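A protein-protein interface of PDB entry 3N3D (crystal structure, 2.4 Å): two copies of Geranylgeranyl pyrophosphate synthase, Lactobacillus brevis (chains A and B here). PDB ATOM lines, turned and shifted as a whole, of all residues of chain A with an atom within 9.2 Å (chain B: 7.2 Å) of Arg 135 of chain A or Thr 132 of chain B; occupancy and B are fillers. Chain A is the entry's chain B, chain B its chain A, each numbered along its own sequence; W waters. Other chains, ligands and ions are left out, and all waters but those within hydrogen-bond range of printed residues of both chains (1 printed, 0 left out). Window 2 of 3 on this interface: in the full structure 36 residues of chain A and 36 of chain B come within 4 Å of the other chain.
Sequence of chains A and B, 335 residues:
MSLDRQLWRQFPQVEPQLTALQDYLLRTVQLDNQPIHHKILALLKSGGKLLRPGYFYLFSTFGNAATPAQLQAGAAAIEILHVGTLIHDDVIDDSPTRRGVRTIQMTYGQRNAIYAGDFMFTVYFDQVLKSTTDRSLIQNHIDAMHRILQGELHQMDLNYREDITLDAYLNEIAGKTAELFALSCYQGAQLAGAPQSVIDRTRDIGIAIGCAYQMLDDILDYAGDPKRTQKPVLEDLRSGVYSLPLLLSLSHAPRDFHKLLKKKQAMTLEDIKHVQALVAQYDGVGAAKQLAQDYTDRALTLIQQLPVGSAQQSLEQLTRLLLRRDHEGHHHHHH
The side-chain carboxylate (OD1) of Asp 126 of chain B is in hydrogen-bond range of the side-chain amide nitrogen (NE2) of Gln 139 of chain A (3.3 Å). The backbone carbonyl oxygen of Leu 129 of chain B sits at hydrogen-bond distance from the guanidinium group of Arg 135 of chain A, at 2.8 Å. The backbone carbonyl oxygen (O) of Leu 129 of chain A is in hydrogen-bond range of the guanidinium group (NH1) of Arg 135 of chain B (2.8 Å).
OG1 of Thr 132 of chain B lies within hydrogen-bond range of N of Asp 134 of chain B, 2.8 Å away. OG1 of Thr 132 of chain A is in hydrogen-bond range of N of Asp 134 of chain A. The side-chain amide nitrogen of Gln 139 of chain A sits at hydrogen-bond distance from the side-chain carboxylate of Asp 143 of chain A (2.8 Å).
Among the printed residues, merely in contact across the chains: Thr 132 of chain A with Arg 135 of chain B, Gln 139 of chain A with Leu 129 of chain B, Arg 135 of chain A with Thr 132 of chain B, Leu 129 of chain A with Ile 138 of chain B, Ile 138 of chain A with Leu 129 of chain B, Ile 142 of chain A with Asp 126 of chain B and Ile 142 of chain A with Leu 129 of chain B.
Arg 135 of chain A touches just these residues of chain B: Leu 129 and Thr 132. Asn 140 of chain A touches none of the printed residues of chain B. Printed residues of chain B within 4 Å of Ile 142 of chain A: Asp 126 and Leu 129. Leu 129 of chain B touches just these residues of chain A: Arg 135, Ile 138, Gln 139 and Ile 142. No residue of chain A comes within 4 Å of Ser 131 of chain B. Thr 132 of chain B touches one residue of chain A. Thr 133 of chain B touches none of the printed residues of chain A. Of the printed residues of chain A, Arg 135 of chain B touches Leu 129 and Thr 132. Ser 136 of chain B touches none of the printed residues of chain A. The nearest residue of chain B that does not touch Arg 135 of chain A is Lys 130 of chain B (4.6 Å). The nearest residue of chain A that does not touch Thr 132 of chain B is Ile 138 of chain A (7.9 Å).
Of the 16 printed residues of chain A, 6 touch a printed residue of chain B. Printed residues of chain A that touch a printed residue of chain B: Leu 129, Thr 132, Arg 135, Ile 138, Gln 139 and Ile 142. Printed residues of chain B that touch a printed residue of chain A: Asp 126, Leu 129, Thr 132, Arg 135 and Ile 138. Hydrophobic or aromatic side chains of chain B that line the printed part of chain A: Leu 129 and Ile 138. Among the printed residues, no Asp or Glu carboxylate lies within 4 Å of a Lys or Arg side-chain nitrogen of the other chain.
Leu 129 of chain A touches Arg 135 of chain B, and with the chains exchanged Arg 135 of chain A touches Leu 129 of chain B. Leu 129 of chain A touches Ile 138 of chain B, and with the chains exchanged Ile 138 of chain A touches Leu 129 of chain B. Thr 132 of chain A touches Arg 135 of chain B, and with the chains exchanged Arg 135 of chain A touches Thr 132 of chain B. Of the 10 pairs that touch across the chains among the printed residues, 6 have their exchanged pair printed and touching as well.
Water W1 bridges OD1 of Asp 126 of chain B (2.6 Å) and OE1 of Gln 139 of chain A (2.8 Å).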
ATOM      1  N   VAL A 128      12.156  18.501  -1.877  1.00  0.00           N
ATOM      2  CA  VAL A 128      11.081  17.785  -2.573  1.00  0.00           C
ATOM      3  C   VAL A 128      10.129  17.169  -1.558  1.00  0.00           C
ATOM      4  O   VAL A 128       8.912  17.400  -1.613  1.00  0.00           O
ATOM      5  CB  VAL A 128      11.622  16.682  -3.512  1.00  0.00           C
ATOM      6  CG1 VAL A 128      10.492  15.769  -3.969  1.00  0.00           C
ATOM      7  CG2 VAL A 128      12.313  17.304  -4.713  1.00  0.00           C
ATOM      8  N   LEU A 129      10.706  16.433  -0.606  1.00  0.00           N
ATOM      9  CA  LEU A 129       9.948  15.738   0.426  1.00  0.00           C
ATOM     10  C   LEU A 129       9.189  16.710   1.307  1.00  0.00           C
ATOM     11  O   LEU A 129       8.049  16.450   1.678  1.00  0.00           O
ATOM     12  CB  LEU A 129      10.862  14.839   1.263  1.00  0.00           C
ATOM     13  CG  LEU A 129      10.160  13.973   2.304  1.00  0.00           C
ATOM     14  CD1 LEU A 129       9.279  12.919   1.627  1.00  0.00           C
ATOM     15  CD2 LEU A 129      11.174  13.343   3.248  1.00  0.00           C
ATOM     16  N   THR A 132       5.827  18.078  -0.693  1.00  0.00           N
ATOM     17  CA  THR A 132       4.670  17.250  -0.949  1.00  0.00           C
ATOM     18  C   THR A 132       4.672  15.961  -0.173  1.00  0.00           C
ATOM     19  O   THR A 132       5.722  15.393   0.140  1.00  0.00           O
ATOM     20  CB  THR A 132       4.434  16.997  -2.470  1.00  0.00           C
ATOM     21  OG1 THR A 132       3.125  16.448  -2.666  1.00  0.00           O
ATOM     22  CG2 THR A 132       5.480  16.078  -3.077  1.00  0.00           C
ATOM     23  N   THR A 133       3.463  15.511   0.120  1.00  0.00           N
ATOM     24  CA  THR A 133       3.238  14.203   0.683  1.00  0.00           C
ATOM     25  C   THR A 133       2.871  13.193  -0.439  1.00  0.00           C
ATOM     26  O   THR A 133       2.964  11.981  -0.241  1.00  0.00           O
ATOM     27  CB  THR A 133       2.169  14.304   1.813  1.00  0.00           C
ATOM     28  OG1 THR A 133       2.456  13.351   2.839  1.00  0.00           O
ATOM     29  CG2 THR A 133       0.731  14.134   1.283  1.00  0.00           C
ATOM     30  N   ASP A 134       2.508  13.720  -1.615  1.00  0.00           N
ATOM     31  CA  ASP A 134       2.026  12.938  -2.768  1.00  0.00           C
ATOM     32  C   ASP A 134       3.136  12.204  -3.514  1.00  0.00           C
ATOM     33  O   ASP A 134       4.051  12.828  -4.050  1.00  0.00           O
ATOM     34  CB  ASP A 134       1.274  13.856  -3.746  1.00  0.00           C
ATOM     35  CG  ASP A 134       0.480  13.086  -4.795  1.00  0.00           C
ATOM     36  OD1 ASP A 134       1.084  12.497  -5.718  1.00  0.00           O
ATOM     37  OD2 ASP A 134      -0.764  13.091  -4.707  1.00  0.00           O
ATOM     38  N   ARG A 135       3.009  10.883  -3.601  1.00  0.00           N
ATOM     39  CA  ARG A 135       4.068  10.041  -4.137  1.00  0.00           C
ATOM     40  C   ARG A 135       4.289  10.161  -5.647  1.00  0.00           C
ATOM     41  O   ARG A 135       5.417   9.984  -6.111  1.00  0.00           O
ATOM     42  CB  ARG A 135       3.911   8.577  -3.669  1.00  0.00           C
ATOM     43  CG  ARG A 135       3.302   7.572  -4.652  1.00  0.00           C
ATOM     44  CD  ARG A 135       4.358   6.697  -5.338  1.00  0.00           C
ATOM     45  NE  ARG A 135       5.213   5.993  -4.379  1.00  0.00           N
ATOM     46  CZ  ARG A 135       4.976   4.778  -3.883  1.00  0.00           C
ATOM     47  NH1 ARG A 135       5.825   4.242  -3.016  1.00  0.00           N
ATOM     48  NH2 ARG A 135       3.897   4.096  -4.248  1.00  0.00           N
ATOM     49  N   SER A 136       3.246  10.464  -6.417  1.00  0.00           N
ATOM     50  CA  SER A 136       3.448  10.619  -7.867  1.00  0.00           C
ATOM     51  C   SER A 136       4.188  11.924  -8.165  1.00  0.00           C
ATOM     52  O   SER A 136       4.981  12.004  -9.107  1.00  0.00           O
ATOM     53  CB  SER A 136       2.141  10.501  -8.662  1.00  0.00           C
ATOM     54  OG  SER A 136       1.194  11.451  -8.226  1.00  0.00           O
ATOM     55  N   LEU A 137       3.953  12.928  -7.326  1.00  0.00           N
ATOM     56  CA  LEU A 137       4.676  14.190  -7.418  1.00  0.00           C
ATOM     57  C   LEU A 137       6.178  14.070  -7.101  1.00  0.00           C
ATOM     58  O   LEU A 137       7.007  14.681  -7.774  1.00  0.00           O
ATOM     59  CB  LEU A 137       4.021  15.221  -6.507  1.00  0.00           C
ATOM     60  CG  LEU A 137       2.889  16.012  -7.146  1.00  0.00           C
ATOM     61  CD1 LEU A 137       2.274  16.957  -6.122  1.00  0.00           C
ATOM     62  CD2 LEU A 137       3.474  16.784  -8.303  1.00  0.00           C
ATOM     63  N   ILE A 138       6.513  13.288  -6.075  1.00  0.00           N
ATOM     64  CA  ILE A 138       7.905  12.967  -5.765  1.00  0.00           C
ATOM     65  C   ILE A 138       8.528  12.177  -6.919  1.00  0.00           C
ATOM     66  O   ILE A 138       9.652  12.464  -7.336  1.00  0.00           O
ATOM     67  CB  ILE A 138       8.027  12.197  -4.419  1.00  0.00           C
ATOM     68  CG1 ILE A 138       7.576  13.087  -3.262  1.00  0.00           C
ATOM     69  CG2 ILE A 138       9.459  11.746  -4.180  1.00  0.00           C
ATOM     70  CD1 ILE A 138       7.133  12.345  -2.002  1.00  0.00           C
ATOM     71  N   GLN A 139       7.771  11.221  -7.460  1.00  0.00           N
ATOM     72  CA  GLN A 139       8.227  10.381  -8.570  1.00  0.00           C
ATOM     73  C   GLN A 139       8.482  11.206  -9.826  1.00  0.00           C
ATOM     74  O   GLN A 139       9.381  10.901 -10.613  1.00  0.00           O
ATOM     75  CB  GLN A 139       7.215   9.261  -8.845  1.00  0.00           C
ATOM     76  CG  GLN A 139       7.627   8.259  -9.931  1.00  0.00           C
ATOM     77  CD  GLN A 139       8.879   7.487  -9.567  1.00  0.00           C
ATOM     78  OE1 GLN A 139       8.928   6.808  -8.543  1.00  0.00           O
ATOM     79  NE2 GLN A 139       9.900   7.593 -10.405  1.00  0.00           N
ATOM     80  N   ASN A 140       7.700  12.271  -9.989  1.00  0.00           N
ATOM     81  CA  ASN A 140       7.875  13.198 -11.100  1.00  0.00           C
ATOM     82  C   ASN A 140       9.225  13.928 -11.032  1.00  0.00           C
ATOM     83  O   ASN A 140       9.925  14.069 -12.048  1.00  0.00           O
ATOM     84  CB  ASN A 140       6.715  14.187 -11.125  1.00  0.00           C
ATOM     85  CG  ASN A 140       6.680  15.001 -12.381  1.00  0.00           C
ATOM     86  OD1 ASN A 140       6.295  14.508 -13.439  1.00  0.00           O
ATOM     87  ND2 ASN A 140       7.085  16.257 -12.282  1.00  0.00           N
ATOM     88  N   HIS A 141       9.594  14.379  -9.833  1.00  0.00           N
ATOM     89  CA  HIS A 141      10.922  14.970  -9.608  1.00  0.00           C
ATOM     90  C   HIS A 141      12.051  13.991  -9.961  1.00  0.00           C
ATOM     91  O   HIS A 141      12.989  14.355 -10.670  1.00  0.00           O
ATOM     92  CB  HIS A 141      11.059  15.421  -8.162  1.00  0.00           C
ATOM     93  CG  HIS A 141      10.645  16.835  -7.925  1.00  0.00           C
ATOM     94  ND1 HIS A 141      11.422  17.911  -8.300  1.00  0.00           N
ATOM     95  CD2 HIS A 141       9.554  17.353  -7.311  1.00  0.00           C
ATOM     96  CE1 HIS A 141      10.817  19.031  -7.946  1.00  0.00           C
ATOM     97  NE2 HIS A 141       9.682  18.721  -7.346  1.00  0.00           N
ATOM     98  N   ILE A 142      11.937  12.749  -9.489  1.00  0.00           N
ATOM     99  CA  ILE A 142      12.944  11.719  -9.747  1.00  0.00           C
ATOM    100  C   ILE A 142      13.122  11.498 -11.245  1.00  0.00           C
ATOM    101  O   ILE A 142      14.238  11.613 -11.744  1.00  0.00           O
ATOM    102  CB  ILE A 142      12.629  10.383  -9.014  1.00  0.00           C
ATOM    103  CG1 ILE A 142      12.622  10.596  -7.504  1.00  0.00           C
ATOM    104  CG2 ILE A 142      13.644   9.294  -9.383  1.00  0.00           C
ATOM    105  CD1 ILE A 142      11.988   9.445  -6.742  1.00  0.00           C
ATOM    106  N   ASP A 143      12.020  11.232 -11.951  1.00  0.00           N
ATOM    107  CA  ASP A 143      12.015  11.050 -13.417  1.00  0.00           C
ATOM    108  C   ASP A 143      12.637  12.217 -14.196  1.00  0.00           C
ATOM    109  O   ASP A 143      13.314  12.007 -15.209  1.00  0.00           O
ATOM    110  CB  ASP A 143      10.585  10.830 -13.932  1.00  0.00           C
ATOM    111  CG  ASP A 143       9.967   9.536 -13.435  1.00  0.00           C
ATOM    112  OD1 ASP A 143       8.736   9.374 -13.608  1.00  0.00           O
ATOM    113  OD2 ASP A 143      10.693   8.689 -12.867  1.00  0.00           O
ATOM    114  N   TYR A 186       4.780  22.027 -14.320  1.00  0.00           N
ATOM    115  CA  TYR A 186       4.004  20.898 -13.827  1.00  0.00           C
ATOM    116  C   TYR A 186       3.854  20.908 -12.316  1.00  0.00           C
ATOM    117  O   TYR A 186       2.729  20.849 -11.820  1.00  0.00           O
ATOM    118  CB  TYR A 186       4.591  19.574 -14.322  1.00  0.00           C
ATOM    119  CG  TYR A 186       3.782  18.351 -13.942  1.00  0.00           C
ATOM    120  CD1 TYR A 186       2.718  17.914 -14.739  1.00  0.00           C
ATOM    121  CD2 TYR A 186       4.087  17.616 -12.791  1.00  0.00           C
ATOM    122  CE1 TYR A 186       1.973  16.784 -14.391  1.00  0.00           C
ATOM    123  CE2 TYR A 186       3.354  16.486 -12.436  1.00  0.00           C
ATOM    124  CZ  TYR A 186       2.301  16.073 -13.240  1.00  0.00           C
ATOM    125  OH  TYR A 186       1.581  14.957 -12.884  1.00  0.00           O
ATOM    126  N   GLN A 187       4.970  20.995 -11.590  1.00  0.00           N
ATOM    127  CA  GLN A 187       4.938  20.928 -10.117  1.00  0.00           C
ATOM    128  C   GLN A 187       4.173  22.094  -9.537  1.00  0.00           C
ATOM    129  O   GLN A 187       3.444  21.928  -8.570  1.00  0.00           O
ATOM    130  CB  GLN A 187       6.346  20.900  -9.515  1.00  0.00           C
ATOM    131  CG  GLN A 187       7.130  19.625  -9.810  1.00  0.00           C
ATOM    132  CD  GLN A 187       6.681  18.442  -8.984  1.00  0.00           C
ATOM    133  OE1 GLN A 187       6.650  17.302  -9.465  1.00  0.00           O
ATOM    134  NE2 GLN A 187       6.336  18.702  -7.732  1.00  0.00           N
ATOM    135  N   GLN B  70       9.246  -4.542  -1.448  1.00  0.00           N
ATOM    136  CA  GLN B  70       9.718  -3.458  -0.593  1.00  0.00           C
ATOM    137  C   GLN B  70      11.137  -3.717  -0.093  1.00  0.00           C
ATOM    138  O   GLN B  70      11.972  -2.807  -0.101  1.00  0.00           O
ATOM    139  CB  GLN B  70       8.828  -3.341   0.629  1.00  0.00           C
ATOM    140  CG  GLN B  70       7.458  -2.725   0.434  1.00  0.00           C
ATOM    141  CD  GLN B  70       6.711  -2.711   1.755  1.00  0.00           C
ATOM    142  OE1 GLN B  70       6.073  -3.695   2.133  1.00  0.00           O
ATOM    143  NE2 GLN B  70       6.833  -1.609   2.490  1.00  0.00           N
ATOM    144  N   ALA B  73      13.683  -3.435  -2.892  1.00  0.00           N
ATOM    145  CA  ALA B  73      13.916  -2.045  -3.256  1.00  0.00           C
ATOM    146  C   ALA B  73      14.797  -1.355  -2.216  1.00  0.00           C
ATOM    147  O   ALA B  73      15.681  -0.577  -2.571  1.00  0.00           O
ATOM    148  CB  ALA B  73      12.601  -1.300  -3.422  1.00  0.00           C
ATOM    149  N   GLY B  74      14.550  -1.660  -0.943  1.00  0.00           N
ATOM    150  CA  GLY B  74      15.309  -1.110   0.165  1.00  0.00           C
ATOM    151  C   GLY B  74      16.753  -1.572   0.147  1.00  0.00           C
ATOM    152  O   GLY B  74      17.657  -0.794   0.438  1.00  0.00           O
ATOM    153  N   ASP B 126      14.810   6.565  -6.473  1.00  0.00           N
ATOM    154  CA  ASP B 126      13.724   5.835  -7.093  1.00  0.00           C
ATOM    155  C   ASP B 126      13.443   4.540  -6.328  1.00  0.00           C
ATOM    156  O   ASP B 126      12.287   4.212  -6.063  1.00  0.00           O
ATOM    157  CB  ASP B 126      14.078   5.547  -8.556  1.00  0.00           C
ATOM    158  CG  ASP B 126      12.958   4.845  -9.310  1.00  0.00           C
ATOM    159  OD1 ASP B 126      11.775   5.189  -9.090  1.00  0.00           O
ATOM    160  OD2 ASP B 126      13.263   3.950 -10.129  1.00  0.00           O
ATOM    161  N   GLN B 127      14.500   3.820  -5.954  1.00  0.00           N
ATOM    162  CA  GLN B 127      14.358   2.608  -5.136  1.00  0.00           C
ATOM    163  C   GLN B 127      13.861   2.903  -3.715  1.00  0.00           C
ATOM    164  O   GLN B 127      13.076   2.133  -3.151  1.00  0.00           O
ATOM    165  CB  GLN B 127      15.673   1.822  -5.084  1.00  0.00           C
ATOM    166  CG  GLN B 127      16.110   1.247  -6.421  1.00  0.00           C
ATOM    167  CD  GLN B 127      15.102   0.253  -7.001  1.00  0.00           C
ATOM    168  OE1 GLN B 127      14.591  -0.606  -6.295  1.00  0.00           O
ATOM    169  NE2 GLN B 127      14.826   0.369  -8.293  1.00  0.00           N
ATOM    170  N   VAL B 128      14.306   4.023  -3.150  1.00  0.00           N
ATOM    171  CA  VAL B 128      13.858   4.456  -1.823  1.00  0.00           C
ATOM    172  C   VAL B 128      12.344   4.646  -1.815  1.00  0.00           C
ATOM    173  O   VAL B 128      11.655   4.149  -0.925  1.00  0.00           O
ATOM    174  CB  VAL B 128      14.581   5.743  -1.381  1.00  0.00           C
ATOM    175  CG1 VAL B 128      13.872   6.420  -0.200  1.00  0.00           C
ATOM    176  CG2 VAL B 128      16.039   5.429  -1.025  1.00  0.00           C
ATOM    177  N   LEU B 129      11.832   5.331  -2.834  1.00  0.00           N
ATOM    178  CA  LEU B 129      10.402   5.552  -2.970  1.00  0.00           C
ATOM    179  C   LEU B 129       9.643   4.248  -3.193  1.00  0.00           C
ATOM    180  O   LEU B 129       8.552   4.058  -2.659  1.00  0.00           O
ATOM    181  CB  LEU B 129      10.128   6.526  -4.106  1.00  0.00           C
ATOM    182  CG  LEU B 129       8.844   7.330  -3.950  1.00  0.00           C
ATOM    183  CD1 LEU B 129       8.939   8.228  -2.717  1.00  0.00           C
ATOM    184  CD2 LEU B 129       8.579   8.140  -5.210  1.00  0.00           C
ATOM    185  N   LYS B 130      10.251   3.328  -3.933  1.00  0.00           N
ATOM    186  CA  LYS B 130       9.651   2.025  -4.191  1.00  0.00           C
ATOM    187  C   LYS B 130       9.599   1.153  -2.927  1.00  0.00           C
ATOM    188  O   LYS B 130       8.733   0.287  -2.797  1.00  0.00           O
ATOM    189  CB  LYS B 130      10.393   1.352  -5.353  1.00  0.00           C
ATOM    190  CG  LYS B 130       9.901  -0.018  -5.768  1.00  0.00           C
ATOM    191  CD  LYS B 130       9.815  -0.172  -7.287  1.00  0.00           C
ATOM    192  CE  LYS B 130      11.123   0.128  -7.994  1.00  0.00           C
ATOM    193  NZ  LYS B 130      10.867   0.466  -9.425  1.00  0.00           N
ATOM    194  N   SER B 131      10.498   1.409  -1.981  1.00  0.00           N
ATOM    195  CA  SER B 131      10.558   0.610  -0.761  1.00  0.00           C
ATOM    196  C   SER B 131       9.518   1.006   0.279  1.00  0.00           C
ATOM    197  O   SER B 131       9.103   0.173   1.082  1.00  0.00           O
ATOM    198  CB  SER B 131      11.963   0.649  -0.148  1.00  0.00           C
ATOM    199  OG  SER B 131      12.230   1.884   0.512  1.00  0.00           O
ATOM    200  N   THR B 132       9.096   2.265   0.280  1.00  0.00           N
ATOM    201  CA  THR B 132       8.270   2.762   1.379  1.00  0.00           C
ATOM    202  C   THR B 132       7.396   3.962   1.022  1.00  0.00           C
ATOM    203  O   THR B 132       7.745   4.782   0.162  1.00  0.00           O
ATOM    204  CB  THR B 132       9.141   3.116   2.636  1.00  0.00           C
ATOM    205  OG1 THR B 132       8.315   3.650   3.672  1.00  0.00           O
ATOM    206  CG2 THR B 132      10.238   4.125   2.311  1.00  0.00           C
ATOM    207  N   THR B 133       6.260   4.045   1.710  1.00  0.00           N
ATOM    208  CA  THR B 133       5.379   5.204   1.658  1.00  0.00           C
ATOM    209  C   THR B 133       5.643   6.102   2.872  1.00  0.00           C
ATOM    210  O   THR B 133       5.321   7.295   2.854  1.00  0.00           O
ATOM    211  CB  THR B 133       3.888   4.787   1.647  1.00  0.00           C
ATOM    212  OG1 THR B 133       3.747   3.478   1.074  1.00  0.00           O
ATOM    213  CG2 THR B 133       3.058   5.792   0.838  1.00  0.00           C
ATOM    214  N   ASP B 134       6.245   5.513   3.906  1.00  0.00           N
ATOM    215  CA  ASP B 134       6.529   6.180   5.179  1.00  0.00           C
ATOM    216  C   ASP B 134       7.584   7.284   5.047  1.00  0.00           C
ATOM    217  O   ASP B 134       8.753   7.023   4.744  1.00  0.00           O
ATOM    218  CB  ASP B 134       6.943   5.133   6.223  1.00  0.00           C
ATOM    219  CG  ASP B 134       7.090   5.701   7.629  1.00  0.00           C
ATOM    220  OD1 ASP B 134       6.935   6.924   7.842  1.00  0.00           O
ATOM    221  OD2 ASP B 134       7.365   4.897   8.544  1.00  0.00           O
ATOM    222  N   ARG B 135       7.152   8.513   5.320  1.00  0.00           N
ATOM    223  CA  ARG B 135       7.957   9.701   5.087  1.00  0.00           C
ATOM    224  C   ARG B 135       9.185   9.860   6.008  1.00  0.00           C
ATOM    225  O   ARG B 135      10.222  10.367   5.572  1.00  0.00           O
ATOM    226  CB  ARG B 135       7.055  10.949   5.029  1.00  0.00           C
ATOM    227  CG  ARG B 135       6.925  11.805   6.279  1.00  0.00           C
ATOM    228  CD  ARG B 135       7.684  13.126   6.126  1.00  0.00           C
ATOM    229  NE  ARG B 135       7.309  13.840   4.901  1.00  0.00           N
ATOM    230  CZ  ARG B 135       6.615  14.977   4.852  1.00  0.00           C
ATOM    231  NH1 ARG B 135       6.336  15.525   3.677  1.00  0.00           N
ATOM    232  NH2 ARG B 135       6.206  15.575   5.967  1.00  0.00           N
ATOM    233  N   SER B 136       9.090   9.402   7.253  1.00  0.00           N
ATOM    234  CA  SER B 136      10.261   9.395   8.147  1.00  0.00           C
ATOM    235  C   SER B 136      11.351   8.436   7.671  1.00  0.00           C
ATOM    236  O   SER B 136      12.533   8.688   7.891  1.00  0.00           O
ATOM    237  CB  SER B 136       9.881   9.104   9.608  1.00  0.00           C
ATOM    238  OG  SER B 136       8.723   8.303   9.682  1.00  0.00           O
ATOM    239  N   LEU B 137      10.958   7.352   7.003  1.00  0.00           N
ATOM    240  CA  LEU B 137      11.934   6.418   6.438  1.00  0.00           C
ATOM    241  C   LEU B 137      12.676   7.010   5.258  1.00  0.00           C
ATOM    242  O   LEU B 137      13.880   6.774   5.085  1.00  0.00           O
ATOM    243  CB  LEU B 137      11.271   5.101   6.047  1.00  0.00           C
ATOM    244  CG  LEU B 137      10.876   4.288   7.273  1.00  0.00           C
ATOM    245  CD1 LEU B 137      10.169   3.006   6.869  1.00  0.00           C
ATOM    246  CD2 LEU B 137      12.131   4.015   8.071  1.00  0.00           C
ATOM    247  N   ILE B 138      11.947   7.787   4.462  1.00  0.00           N
ATOM    248  CA  ILE B 138      12.529   8.536   3.369  1.00  0.00           C
ATOM    249  C   ILE B 138      13.474   9.604   3.923  1.00  0.00           C
ATOM    250  O   ILE B 138      14.609   9.714   3.467  1.00  0.00           O
ATOM    251  CB  ILE B 138      11.427   9.122   2.446  1.00  0.00           C
ATOM    252  CG1 ILE B 138      10.682   7.973   1.751  1.00  0.00           C
ATOM    253  CG2 ILE B 138      12.017  10.098   1.424  1.00  0.00           C
ATOM    254  CD1 ILE B 138       9.364   8.365   1.118  1.00  0.00           C
ATOM    255  N   HIS B 141      16.782   8.275   5.018  1.00  0.00           N
ATOM    256  CA  HIS B 141      17.699   8.069   3.889  1.00  0.00           C
ATOM    257  C   HIS B 141      18.416   9.368   3.514  1.00  0.00           C
ATOM    258  O   HIS B 141      19.612   9.358   3.224  1.00  0.00           O
ATOM    259  CB  HIS B 141      16.948   7.554   2.658  1.00  0.00           C
ATOM    260  CG  HIS B 141      16.914   6.064   2.539  1.00  0.00           C
ATOM    261  ND1 HIS B 141      18.008   5.322   2.141  1.00  0.00           N
ATOM    262  CD2 HIS B 141      15.908   5.178   2.735  1.00  0.00           C
ATOM    263  CE1 HIS B 141      17.679   4.042   2.110  1.00  0.00           C
ATOM    264  NE2 HIS B 141      16.412   3.928   2.471  1.00  0.00           N
ATOM    265  N   GLN B 187      16.930   0.481   8.191  1.00  0.00           N
ATOM    266  CA  GLN B 187      15.873   0.404   7.184  1.00  0.00           C
ATOM    267  C   GLN B 187      15.273  -0.997   7.137  1.00  0.00           C
ATOM    268  O   GLN B 187      14.056  -1.144   7.119  1.00  0.00           O
ATOM    269  CB  GLN B 187      16.383   0.822   5.800  1.00  0.00           C
ATOM    270  CG  GLN B 187      16.693   2.304   5.660  1.00  0.00           C
ATOM    271  CD  GLN B 187      15.459   3.190   5.610  1.00  0.00           C
ATOM    272  OE1 GLN B 187      15.435   4.269   6.206  1.00  0.00           O
ATOM    273  NE2 GLN B 187      14.437   2.751   4.884  1.00  0.00           N
ATOM    274  N   LEU B 191      11.419  -1.261   7.971  1.00  0.00           N
ATOM    275  CA  LEU B 191      10.495  -1.649   6.889  1.00  0.00           C
ATOM    276  C   LEU B 191       9.699  -2.882   7.276  1.00  0.00           C
ATOM    277  O   LEU B 191       8.485  -2.941   7.076  1.00  0.00           O
ATOM    278  CB  LEU B 191      11.224  -1.921   5.567  1.00  0.00           C
ATOM    279  CG  LEU B 191      11.772  -0.741   4.762  1.00  0.00           C
ATOM    280  CD1 LEU B 191      12.563  -1.292   3.610  1.00  0.00           C
ATOM    281  CD2 LEU B 191      10.668   0.176   4.262  1.00  0.00           C
HETATM  282  O   HOH W   1       9.896   4.444  -7.505  1.00  0.00           O
